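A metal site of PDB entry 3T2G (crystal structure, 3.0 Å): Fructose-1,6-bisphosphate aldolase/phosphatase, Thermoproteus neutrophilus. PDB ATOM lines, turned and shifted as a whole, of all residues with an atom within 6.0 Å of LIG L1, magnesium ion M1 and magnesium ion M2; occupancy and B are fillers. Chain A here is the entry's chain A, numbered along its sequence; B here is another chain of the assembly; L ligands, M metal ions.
Magnesium ion M2 is bound by OD2 of Asp 11 (2.2 Å), OD2 of Asp 52 (2.3 Å), ND1 of His 18 (2.4 Å) and O3 of LIG L1 (2.4 Å). Magnesium ion M2 has four donor atoms within binding distance. Slightly farther from magnesium ion M2 lies the side-chain amide oxygen (OE1) of Gln 95 (2.8 Å).
The side-chain carboxylate (OD2) of Asp 53 sits close to the side-chain carboxylate (OD2) of Asp 234 (2.7 Å). The side-chain carboxylate (OD1) of Asp 234 is in hydrogen-bond range of the backbone NH (N) of Lys 133, 3.3 Å away. The backbone carbonyl oxygen (O) of Asp 234 lies close to the side-chain amino group (NZ) of Lys 9 (3.2 Å). The side-chain carboxylate (OD1) of Asp 52 lies close to the side-chain amino group (NZ) of Lys 133, at 3.4 Å. The side-chain amino group of Lys 133 is in salt-bridge range of the side-chain carboxylate of Asp 132 (3.0 Å). OD1 of Asp 53 is in salt-bridge range of NZ of Lys 9 (3.1 Å). SD of Met 265 lies close to NE of Arg 266 (3.7 Å). The backbone NH (N) of Trp 264 is in hydrogen-bond range of the backbone carbonyl oxygen (O) of Lys 133.
The side-chain carboxylate (OD1) of Asp 233 sits close to an oxygen (O1) of LIG L1 (2.6 Å). An oxygen (O6) of LIG L1 lies within hydrogen-bond range of the backbone NH (N) of Arg 266, at 2.7 Å. The side-chain amino group (NZ) of Lys 133 sits close to an oxygen (O2) of LIG L1 (2.9 Å). The side-chain carboxylate of Asp 297 lies within hydrogen-bond range of an oxygen (O6) of LIG L1, 2.9 Å away. The backbone NH of Gly 267 is in hydrogen-bond range of an oxygen (O5) of LIG L1, 3.2 Å away. NH1 of Arg 266 lies within salt-bridge range of O2 of LG2 L2. The side-chain hydroxyl (OH) of Tyr 91 sits at hydrogen-bond distance from an oxygen (O3) of LG2 L2, at 2.7 Å.
The nearest printed residue that does not touch magnesium ion M2 is Gly 17 (4.9 Å).
Trp 264 touches LIG L1. CA of Met 265 touches O6 of LIG L1, at 3.7 Å. The nearest printed residue that does not touch LIG L1 is Asp 53 (4.5 Å).
The side-chain carboxylate (OD2) of Asp 234 binds magnesium ion M1, 2.0 Å away. An oxygen (O2) of LIG L1 is bound to magnesium ion M1 (2.0 Å). Magnesium ion M1 is bound by OD1 of Asp 52 (2.0 Å). Magnesium ion M1 is bound by OD1 of Asp 132 (2.4 Å). Magnesium ion M1 has four donor atoms within binding distance. Slightly farther from magnesium ion M1 lies the side-chain carboxylate (OD2) of Asp 53 (2.7 Å).
An oxygen (O6) of LIG L1 sits close to an oxygen (O5) of LG2 L2, at 3.5 Å.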
ATOM      1  N   LYS A   9     -23.731  -7.544   7.828  1.00  0.00           N
ATOM      2  CA  LYS A   9     -23.783  -6.159   7.398  1.00  0.00           C
ATOM      3  C   LYS A   9     -23.692  -6.003   5.885  1.00  0.00           C
ATOM      4  O   LYS A   9     -22.975  -6.750   5.225  1.00  0.00           O
ATOM      5  CB  LYS A   9     -22.620  -5.429   8.077  1.00  0.00           C
ATOM      6  CG  LYS A   9     -22.495  -3.966   7.783  1.00  0.00           C
ATOM      7  CD  LYS A   9     -21.225  -3.651   6.972  1.00  0.00           C
ATOM      8  CE  LYS A   9     -21.332  -4.035   5.524  1.00  0.00           C
ATOM      9  NZ  LYS A   9     -20.292  -3.414   4.662  1.00  0.00           N
ATOM     10  N   ASP A  11     -23.956  -2.857   2.461  1.00  0.00           N
ATOM     11  CA  ASP A  11     -24.372  -1.613   1.834  1.00  0.00           C
ATOM     12  C   ASP A  11     -25.249  -1.984   0.630  1.00  0.00           C
ATOM     13  O   ASP A  11     -24.772  -2.603  -0.328  1.00  0.00           O
ATOM     14  CB  ASP A  11     -23.138  -0.827   1.436  1.00  0.00           C
ATOM     15  CG  ASP A  11     -23.458   0.489   0.718  1.00  0.00           C
ATOM     16  OD1 ASP A  11     -24.616   0.749   0.289  1.00  0.00           O
ATOM     17  OD2 ASP A  11     -22.496   1.284   0.573  1.00  0.00           O
ATOM     18  N   GLY A  14     -27.440   3.839  -1.053  1.00  0.00           N
ATOM     19  CA  GLY A  14     -27.118   5.064  -0.335  1.00  0.00           C
ATOM     20  C   GLY A  14     -28.047   6.217  -0.684  1.00  0.00           C
ATOM     21  O   GLY A  14     -28.554   6.327  -1.803  1.00  0.00           O
ATOM     22  N   GLY A  17     -26.102   9.383  -2.594  1.00  0.00           N
ATOM     23  CA  GLY A  17     -24.761   8.850  -2.827  1.00  0.00           C
ATOM     24  C   GLY A  17     -24.359   7.880  -1.737  1.00  0.00           C
ATOM     25  O   GLY A  17     -24.935   6.828  -1.625  1.00  0.00           O
ATOM     26  N   HIS A  18     -23.394   8.270  -0.906  1.00  0.00           N
ATOM     27  CA  HIS A  18     -22.792   7.353   0.068  1.00  0.00           C
ATOM     28  C   HIS A  18     -22.955   7.842   1.524  1.00  0.00           C
ATOM     29  O   HIS A  18     -22.327   7.320   2.460  1.00  0.00           O
ATOM     30  CB  HIS A  18     -21.328   7.093  -0.289  1.00  0.00           C
ATOM     31  CG  HIS A  18     -21.138   6.313  -1.563  1.00  0.00           C
ATOM     32  ND1 HIS A  18     -21.744   5.094  -1.786  1.00  0.00           N
ATOM     33  CD2 HIS A  18     -20.417   6.577  -2.667  1.00  0.00           C
ATOM     34  CE1 HIS A  18     -21.408   4.645  -2.981  1.00  0.00           C
ATOM     35  NE2 HIS A  18     -20.590   5.525  -3.539  1.00  0.00           N
ATOM     36  N   VAL A  50     -24.706   2.522  10.247  1.00  0.00           N
ATOM     37  CA  VAL A  50     -23.749   3.629  10.377  1.00  0.00           C
ATOM     38  C   VAL A  50     -23.340   4.043   8.981  1.00  0.00           C
ATOM     39  O   VAL A  50     -22.924   3.207   8.189  1.00  0.00           O
ATOM     40  CB  VAL A  50     -22.482   3.242  11.157  1.00  0.00           C
ATOM     41  CG1 VAL A  50     -21.447   4.365  11.093  1.00  0.00           C
ATOM     42  CG2 VAL A  50     -22.813   2.894  12.626  1.00  0.00           C
ATOM     43  N   GLY A  51     -23.469   5.327   8.668  1.00  0.00           N
ATOM     44  CA  GLY A  51     -23.277   5.784   7.297  1.00  0.00           C
ATOM     45  C   GLY A  51     -24.250   4.994   6.420  1.00  0.00           C
ATOM     46  O   GLY A  51     -25.471   5.027   6.658  1.00  0.00           O
ATOM     47  N   ASP A  52     -23.728   4.247   5.458  1.00  0.00           N
ATOM     48  CA  ASP A  52     -24.588   3.638   4.465  1.00  0.00           C
ATOM     49  C   ASP A  52     -24.602   2.106   4.519  1.00  0.00           C
ATOM     50  O   ASP A  52     -25.029   1.437   3.557  1.00  0.00           O
ATOM     51  CB  ASP A  52     -24.257   4.160   3.065  1.00  0.00           C
ATOM     52  CG  ASP A  52     -22.865   3.762   2.580  1.00  0.00           C
ATOM     53  OD1 ASP A  52     -22.044   3.250   3.383  1.00  0.00           O
ATOM     54  OD2 ASP A  52     -22.585   3.968   1.371  1.00  0.00           O
ATOM     55  N   ASP A  53     -24.156   1.555   5.649  1.00  0.00           N
ATOM     56  CA  ASP A  53     -24.131   0.105   5.820  1.00  0.00           C
ATOM     57  C   ASP A  53     -25.191  -0.321   6.796  1.00  0.00           C
ATOM     58  O   ASP A  53     -25.234   0.176   7.941  1.00  0.00           O
ATOM     59  CB  ASP A  53     -22.785  -0.380   6.345  1.00  0.00           C
ATOM     60  CG  ASP A  53     -21.652   0.037   5.462  1.00  0.00           C
ATOM     61  OD1 ASP A  53     -21.476  -0.545   4.352  1.00  0.00           O
ATOM     62  OD2 ASP A  53     -20.942   0.981   5.900  1.00  0.00           O
ATOM     63  N   TYR A  91     -28.405   5.207  -4.480  1.00  0.00           N
ATOM     64  CA  TYR A  91     -27.063   5.150  -5.040  1.00  0.00           C
ATOM     65  C   TYR A  91     -26.264   3.934  -4.611  1.00  0.00           C
ATOM     66  O   TYR A  91     -26.070   3.706  -3.415  1.00  0.00           O
ATOM     67  CB  TYR A  91     -26.257   6.431  -4.799  1.00  0.00           C
ATOM     68  CG  TYR A  91     -25.060   6.482  -5.718  1.00  0.00           C
ATOM     69  CD1 TYR A  91     -25.134   7.163  -6.928  1.00  0.00           C
ATOM     70  CD2 TYR A  91     -23.879   5.802  -5.394  1.00  0.00           C
ATOM     71  CE1 TYR A  91     -24.064   7.177  -7.797  1.00  0.00           C
ATOM     72  CE2 TYR A  91     -22.807   5.809  -6.270  1.00  0.00           C
ATOM     73  CZ  TYR A  91     -22.907   6.500  -7.454  1.00  0.00           C
ATOM     74  OH  TYR A  91     -21.855   6.501  -8.317  1.00  0.00           O
ATOM     75  N   GLY A  92     -25.779   3.207  -5.614  1.00  0.00           N
ATOM     76  CA  GLY A  92     -25.066   1.938  -5.423  1.00  0.00           C
ATOM     77  C   GLY A  92     -26.026   0.941  -4.822  1.00  0.00           C
ATOM     78  O   GLY A  92     -25.682   0.225  -3.884  1.00  0.00           O
ATOM     79  N   GLN A  95     -25.266  -2.805  -3.804  1.00  0.00           N
ATOM     80  CA  GLN A  95     -23.808  -2.679  -3.959  1.00  0.00           C
ATOM     81  C   GLN A  95     -23.061  -3.932  -3.509  1.00  0.00           C
ATOM     82  O   GLN A  95     -22.303  -4.506  -4.275  1.00  0.00           O
ATOM     83  CB  GLN A  95     -23.301  -1.475  -3.193  1.00  0.00           C
ATOM     84  CG  GLN A  95     -22.232  -0.686  -3.885  1.00  0.00           C
ATOM     85  CD  GLN A  95     -21.520   0.196  -2.897  1.00  0.00           C
ATOM     86  OE1 GLN A  95     -21.683   1.435  -2.895  1.00  0.00           O
ATOM     87  NE2 GLN A  95     -20.766  -0.441  -2.010  1.00  0.00           N
ATOM     88  N   ASP A 132     -18.246   2.895   9.250  1.00  0.00           N
ATOM     89  CA  ASP A 132     -18.477   3.173   7.832  1.00  0.00           C
ATOM     90  C   ASP A 132     -17.288   3.929   7.269  1.00  0.00           C
ATOM     91  O   ASP A 132     -16.616   4.659   8.011  1.00  0.00           O
ATOM     92  CB  ASP A 132     -19.735   4.003   7.600  1.00  0.00           C
ATOM     93  CG  ASP A 132     -20.067   4.124   6.110  1.00  0.00           C
ATOM     94  OD1 ASP A 132     -19.856   3.136   5.372  1.00  0.00           O
ATOM     95  OD2 ASP A 132     -20.541   5.199   5.659  1.00  0.00           O
ATOM     96  N   LYS A 133     -17.038   3.746   5.975  1.00  0.00           N
ATOM     97  CA  LYS A 133     -16.039   4.524   5.264  1.00  0.00           C
ATOM     98  C   LYS A 133     -14.615   4.139   5.658  1.00  0.00           C
ATOM     99  O   LYS A 133     -13.686   4.917   5.470  1.00  0.00           O
ATOM    100  CB  LYS A 133     -16.276   6.006   5.479  1.00  0.00           C
ATOM    101  CG  LYS A 133     -16.795   6.688   4.272  1.00  0.00           C
ATOM    102  CD  LYS A 133     -18.283   6.590   4.199  1.00  0.00           C
ATOM    103  CE  LYS A 133     -18.797   6.558   2.758  1.00  0.00           C
ATOM    104  NZ  LYS A 133     -20.213   6.109   2.814  1.00  0.00           N
ATOM    105  N   THR A 134     -14.453   2.940   6.194  1.00  0.00           N
ATOM    106  CA  THR A 134     -13.159   2.391   6.528  1.00  0.00           C
ATOM    107  C   THR A 134     -13.107   0.920   6.133  1.00  0.00           C
ATOM    108  O   THR A 134     -13.938   0.471   5.369  1.00  0.00           O
ATOM    109  CB  THR A 134     -12.843   2.565   8.016  1.00  0.00           C
ATOM    110  OG1 THR A 134     -11.446   2.315   8.251  1.00  0.00           O
ATOM    111  CG2 THR A 134     -13.709   1.616   8.913  1.00  0.00           C
ATOM    112  N   ASP A 233     -15.178  -4.167   3.017  1.00  0.00           N
ATOM    113  CA  ASP A 233     -15.307  -2.768   3.349  1.00  0.00           C
ATOM    114  C   ASP A 233     -16.087  -2.704   4.636  1.00  0.00           C
ATOM    115  O   ASP A 233     -16.595  -3.702   5.106  1.00  0.00           O
ATOM    116  CB  ASP A 233     -16.011  -1.964   2.235  1.00  0.00           C
ATOM    117  CG  ASP A 233     -15.248  -0.679   1.866  1.00  0.00           C
ATOM    118  OD1 ASP A 233     -15.772   0.110   1.033  1.00  0.00           O
ATOM    119  OD2 ASP A 233     -14.107  -0.474   2.382  1.00  0.00           O
ATOM    120  N   ASP A 234     -16.128  -1.508   5.204  1.00  0.00           N
ATOM    121  CA  ASP A 234     -16.881  -1.139   6.398  1.00  0.00           C
ATOM    122  C   ASP A 234     -17.244  -2.342   7.279  1.00  0.00           C
ATOM    123  O   ASP A 234     -18.296  -2.948   7.090  1.00  0.00           O
ATOM    124  CB  ASP A 234     -18.112  -0.330   5.992  1.00  0.00           C
ATOM    125  CG  ASP A 234     -17.877   0.560   4.774  1.00  0.00           C
ATOM    126  OD1 ASP A 234     -16.723   0.864   4.411  1.00  0.00           O
ATOM    127  OD2 ASP A 234     -18.873   0.968   4.145  1.00  0.00           O
ATOM    128  N   TRP A 264     -12.120   6.399   4.082  1.00  0.00           N
ATOM    129  CA  TRP A 264     -12.681   7.700   3.808  1.00  0.00           C
ATOM    130  C   TRP A 264     -13.065   7.723   2.330  1.00  0.00           C
ATOM    131  O   TRP A 264     -13.607   6.739   1.789  1.00  0.00           O
ATOM    132  CB  TRP A 264     -11.677   8.854   4.115  1.00  0.00           C
ATOM    133  CG  TRP A 264     -12.345  10.143   4.539  1.00  0.00           C
ATOM    134  CD1 TRP A 264     -13.649  10.483   4.353  1.00  0.00           C
ATOM    135  CD2 TRP A 264     -11.730  11.266   5.208  1.00  0.00           C
ATOM    136  NE1 TRP A 264     -13.908  11.736   4.881  1.00  0.00           N
ATOM    137  CE2 TRP A 264     -12.745  12.243   5.404  1.00  0.00           C
ATOM    138  CE3 TRP A 264     -10.424  11.555   5.652  1.00  0.00           C
ATOM    139  CZ2 TRP A 264     -12.498  13.485   6.035  1.00  0.00           C
ATOM    140  CZ3 TRP A 264     -10.186  12.793   6.282  1.00  0.00           C
ATOM    141  CH2 TRP A 264     -11.219  13.732   6.467  1.00  0.00           C
ATOM    142  N   MET A 265     -12.731   8.824   1.670  1.00  0.00           N
ATOM    143  CA  MET A 265     -13.268   9.142   0.370  1.00  0.00           C
ATOM    144  C   MET A 265     -12.638   8.346  -0.728  1.00  0.00           C
ATOM    145  O   MET A 265     -11.416   8.429  -0.941  1.00  0.00           O
ATOM    146  CB  MET A 265     -13.051  10.615   0.091  1.00  0.00           C
ATOM    147  CG  MET A 265     -12.970  10.977  -1.366  1.00  0.00           C
ATOM    148  SD  MET A 265     -14.536  10.927  -2.249  1.00  0.00           S
ATOM    149  CE  MET A 265     -15.618  12.010  -1.299  1.00  0.00           C
ATOM    150  N   ARG A 266     -13.496   7.596  -1.420  1.00  0.00           N
ATOM    151  CA  ARG A 266     -13.119   6.706  -2.524  1.00  0.00           C
ATOM    152  C   ARG A 266     -12.235   5.523  -2.126  1.00  0.00           C
ATOM    153  O   ARG A 266     -11.563   4.933  -2.962  1.00  0.00           O
ATOM    154  CB  ARG A 266     -12.514   7.467  -3.674  1.00  0.00           C
ATOM    155  CG  ARG A 266     -13.446   8.503  -4.212  1.00  0.00           C
ATOM    156  CD  ARG A 266     -12.735   9.363  -5.220  1.00  0.00           C
ATOM    157  NE  ARG A 266     -13.625  10.373  -5.772  1.00  0.00           N
ATOM    158  CZ  ARG A 266     -14.293  10.247  -6.911  1.00  0.00           C
ATOM    159  NH1 ARG A 266     -14.162   9.155  -7.659  1.00  0.00           N
ATOM    160  NH2 ARG A 266     -15.082  11.245  -7.303  1.00  0.00           N
ATOM    161  N   GLY A 267     -12.300   5.173  -0.840  1.00  0.00           N
ATOM    162  CA  GLY A 267     -11.544   4.059  -0.275  1.00  0.00           C
ATOM    163  C   GLY A 267     -10.045   4.225  -0.458  1.00  0.00           C
ATOM    164  O   GLY A 267      -9.320   3.232  -0.493  1.00  0.00           O
ATOM    165  N   SER A 268      -9.605   5.477  -0.531  1.00  0.00           N
ATOM    166  CA  SER A 268      -8.247   5.783  -0.948  1.00  0.00           C
ATOM    167  C   SER A 268      -7.494   6.817  -0.108  1.00  0.00           C
ATOM    168  O   SER A 268      -6.400   7.300  -0.502  1.00  0.00           O
ATOM    169  CB  SER A 268      -8.259   6.203  -2.419  1.00  0.00           C
ATOM    170  OG  SER A 268      -9.019   5.264  -3.148  1.00  0.00           O
ATOM    171  N   PHE A 296     -16.058  15.281   2.640  1.00  0.00           N
ATOM    172  CA  PHE A 296     -15.212  14.314   1.978  1.00  0.00           C
ATOM    173  C   PHE A 296     -15.694  12.867   2.103  1.00  0.00           C
ATOM    174  O   PHE A 296     -14.905  11.963   1.894  1.00  0.00           O
ATOM    175  CB  PHE A 296     -13.770  14.441   2.501  1.00  0.00           C
ATOM    176  CG  PHE A 296     -12.710  14.078   1.476  1.00  0.00           C
ATOM    177  CD1 PHE A 296     -12.743  14.620   0.191  1.00  0.00           C
ATOM    178  CD2 PHE A 296     -11.671  13.224   1.811  1.00  0.00           C
ATOM    179  CE1 PHE A 296     -11.790  14.307  -0.749  1.00  0.00           C
ATOM    180  CE2 PHE A 296     -10.698  12.912   0.881  1.00  0.00           C
ATOM    181  CZ  PHE A 296     -10.760  13.450  -0.414  1.00  0.00           C
ATOM    182  N   ASP A 297     -16.990  12.648   2.396  1.00  0.00           N
ATOM    183  CA  ASP A 297     -17.556  11.301   2.639  1.00  0.00           C
ATOM    184  C   ASP A 297     -17.075  10.655   3.931  1.00  0.00           C
ATOM    185  O   ASP A 297     -16.692   9.479   3.956  1.00  0.00           O
ATOM    186  CB  ASP A 297     -17.281  10.312   1.507  1.00  0.00           C
ATOM    187  CG  ASP A 297     -18.177  10.512   0.344  1.00  0.00           C
ATOM    188  OD1 ASP A 297     -19.120  11.327   0.442  1.00  0.00           O
ATOM    189  OD2 ASP A 297     -17.925   9.852  -0.687  1.00  0.00           O
ATOM    190  N   ALA B 247     -18.051  13.284  -6.132  1.00  0.00           N
ATOM    191  CA  ALA B 247     -18.751  12.538  -5.092  1.00  0.00           C
ATOM    192  C   ALA B 247     -19.547  13.555  -4.288  1.00  0.00           C
ATOM    193  O   ALA B 247     -19.222  14.762  -4.296  1.00  0.00           O
ATOM    194  CB  ALA B 247     -17.763  11.806  -4.209  1.00  0.00           C
HETATM  195  P1  LIG L   1     -18.833   2.816   1.215  1.00  0.00           P
HETATM  196  O1  LIG L   1     -17.682   1.867   1.456  1.00  0.00           O
HETATM  197  O2  LIG L   1     -19.388   3.398   2.491  1.00  0.00           O
HETATM  198  O3  LIG L   1     -19.895   2.366   0.231  1.00  0.00           O
HETATM  199  O4  LIG L   1     -18.094   4.071   0.511  1.00  0.00           O
HETATM  200  C1  LIG L   1     -17.503   3.942  -0.786  1.00  0.00           C
HETATM  201  C2  LIG L   1     -16.633   5.121  -1.092  1.00  0.00           C
HETATM  202  O5  LIG L   1     -15.472   4.938  -1.405  1.00  0.00           O
HETATM  203  C3  LIG L   1     -17.219   6.505  -1.020  1.00  0.00           C
HETATM  204  O6  LIG L   1     -16.216   7.509  -1.104  1.00  0.00           O
HETATM  205  P1  LG2 L   2     -18.648   6.925  -7.832  1.00  0.00           P
HETATM  206  O1  LG2 L   2     -19.498   8.157  -8.011  1.00  0.00           O
HETATM  207  O2  LG2 L   2     -17.296   6.948  -8.499  1.00  0.00           O
HETATM  208  O3  LG2 L   2     -19.398   5.605  -7.887  1.00  0.00           O
HETATM  209  O4  LG2 L   2     -18.236   7.056  -6.296  1.00  0.00           O
HETATM  210  C1  LG2 L   2     -17.682   8.253  -5.762  1.00  0.00           C
HETATM  211  C2  LG2 L   2     -17.728   7.972  -4.289  1.00  0.00           C
HETATM  212  O5  LG2 L   2     -18.413   8.643  -3.540  1.00  0.00           O
HETATM  213  C3  LG2 L   2     -16.956   6.788  -3.779  1.00  0.00           C
HETATM  214  O6  LG2 L   2     -16.463   5.956  -4.850  1.00  0.00           O
HETATM  215 MG    MG M   1     -20.477   1.956   3.417  1.00  0.00          MG
HETATM  216 MG    MG M   2     -22.040   3.040  -0.634  1.00  0.00          MG
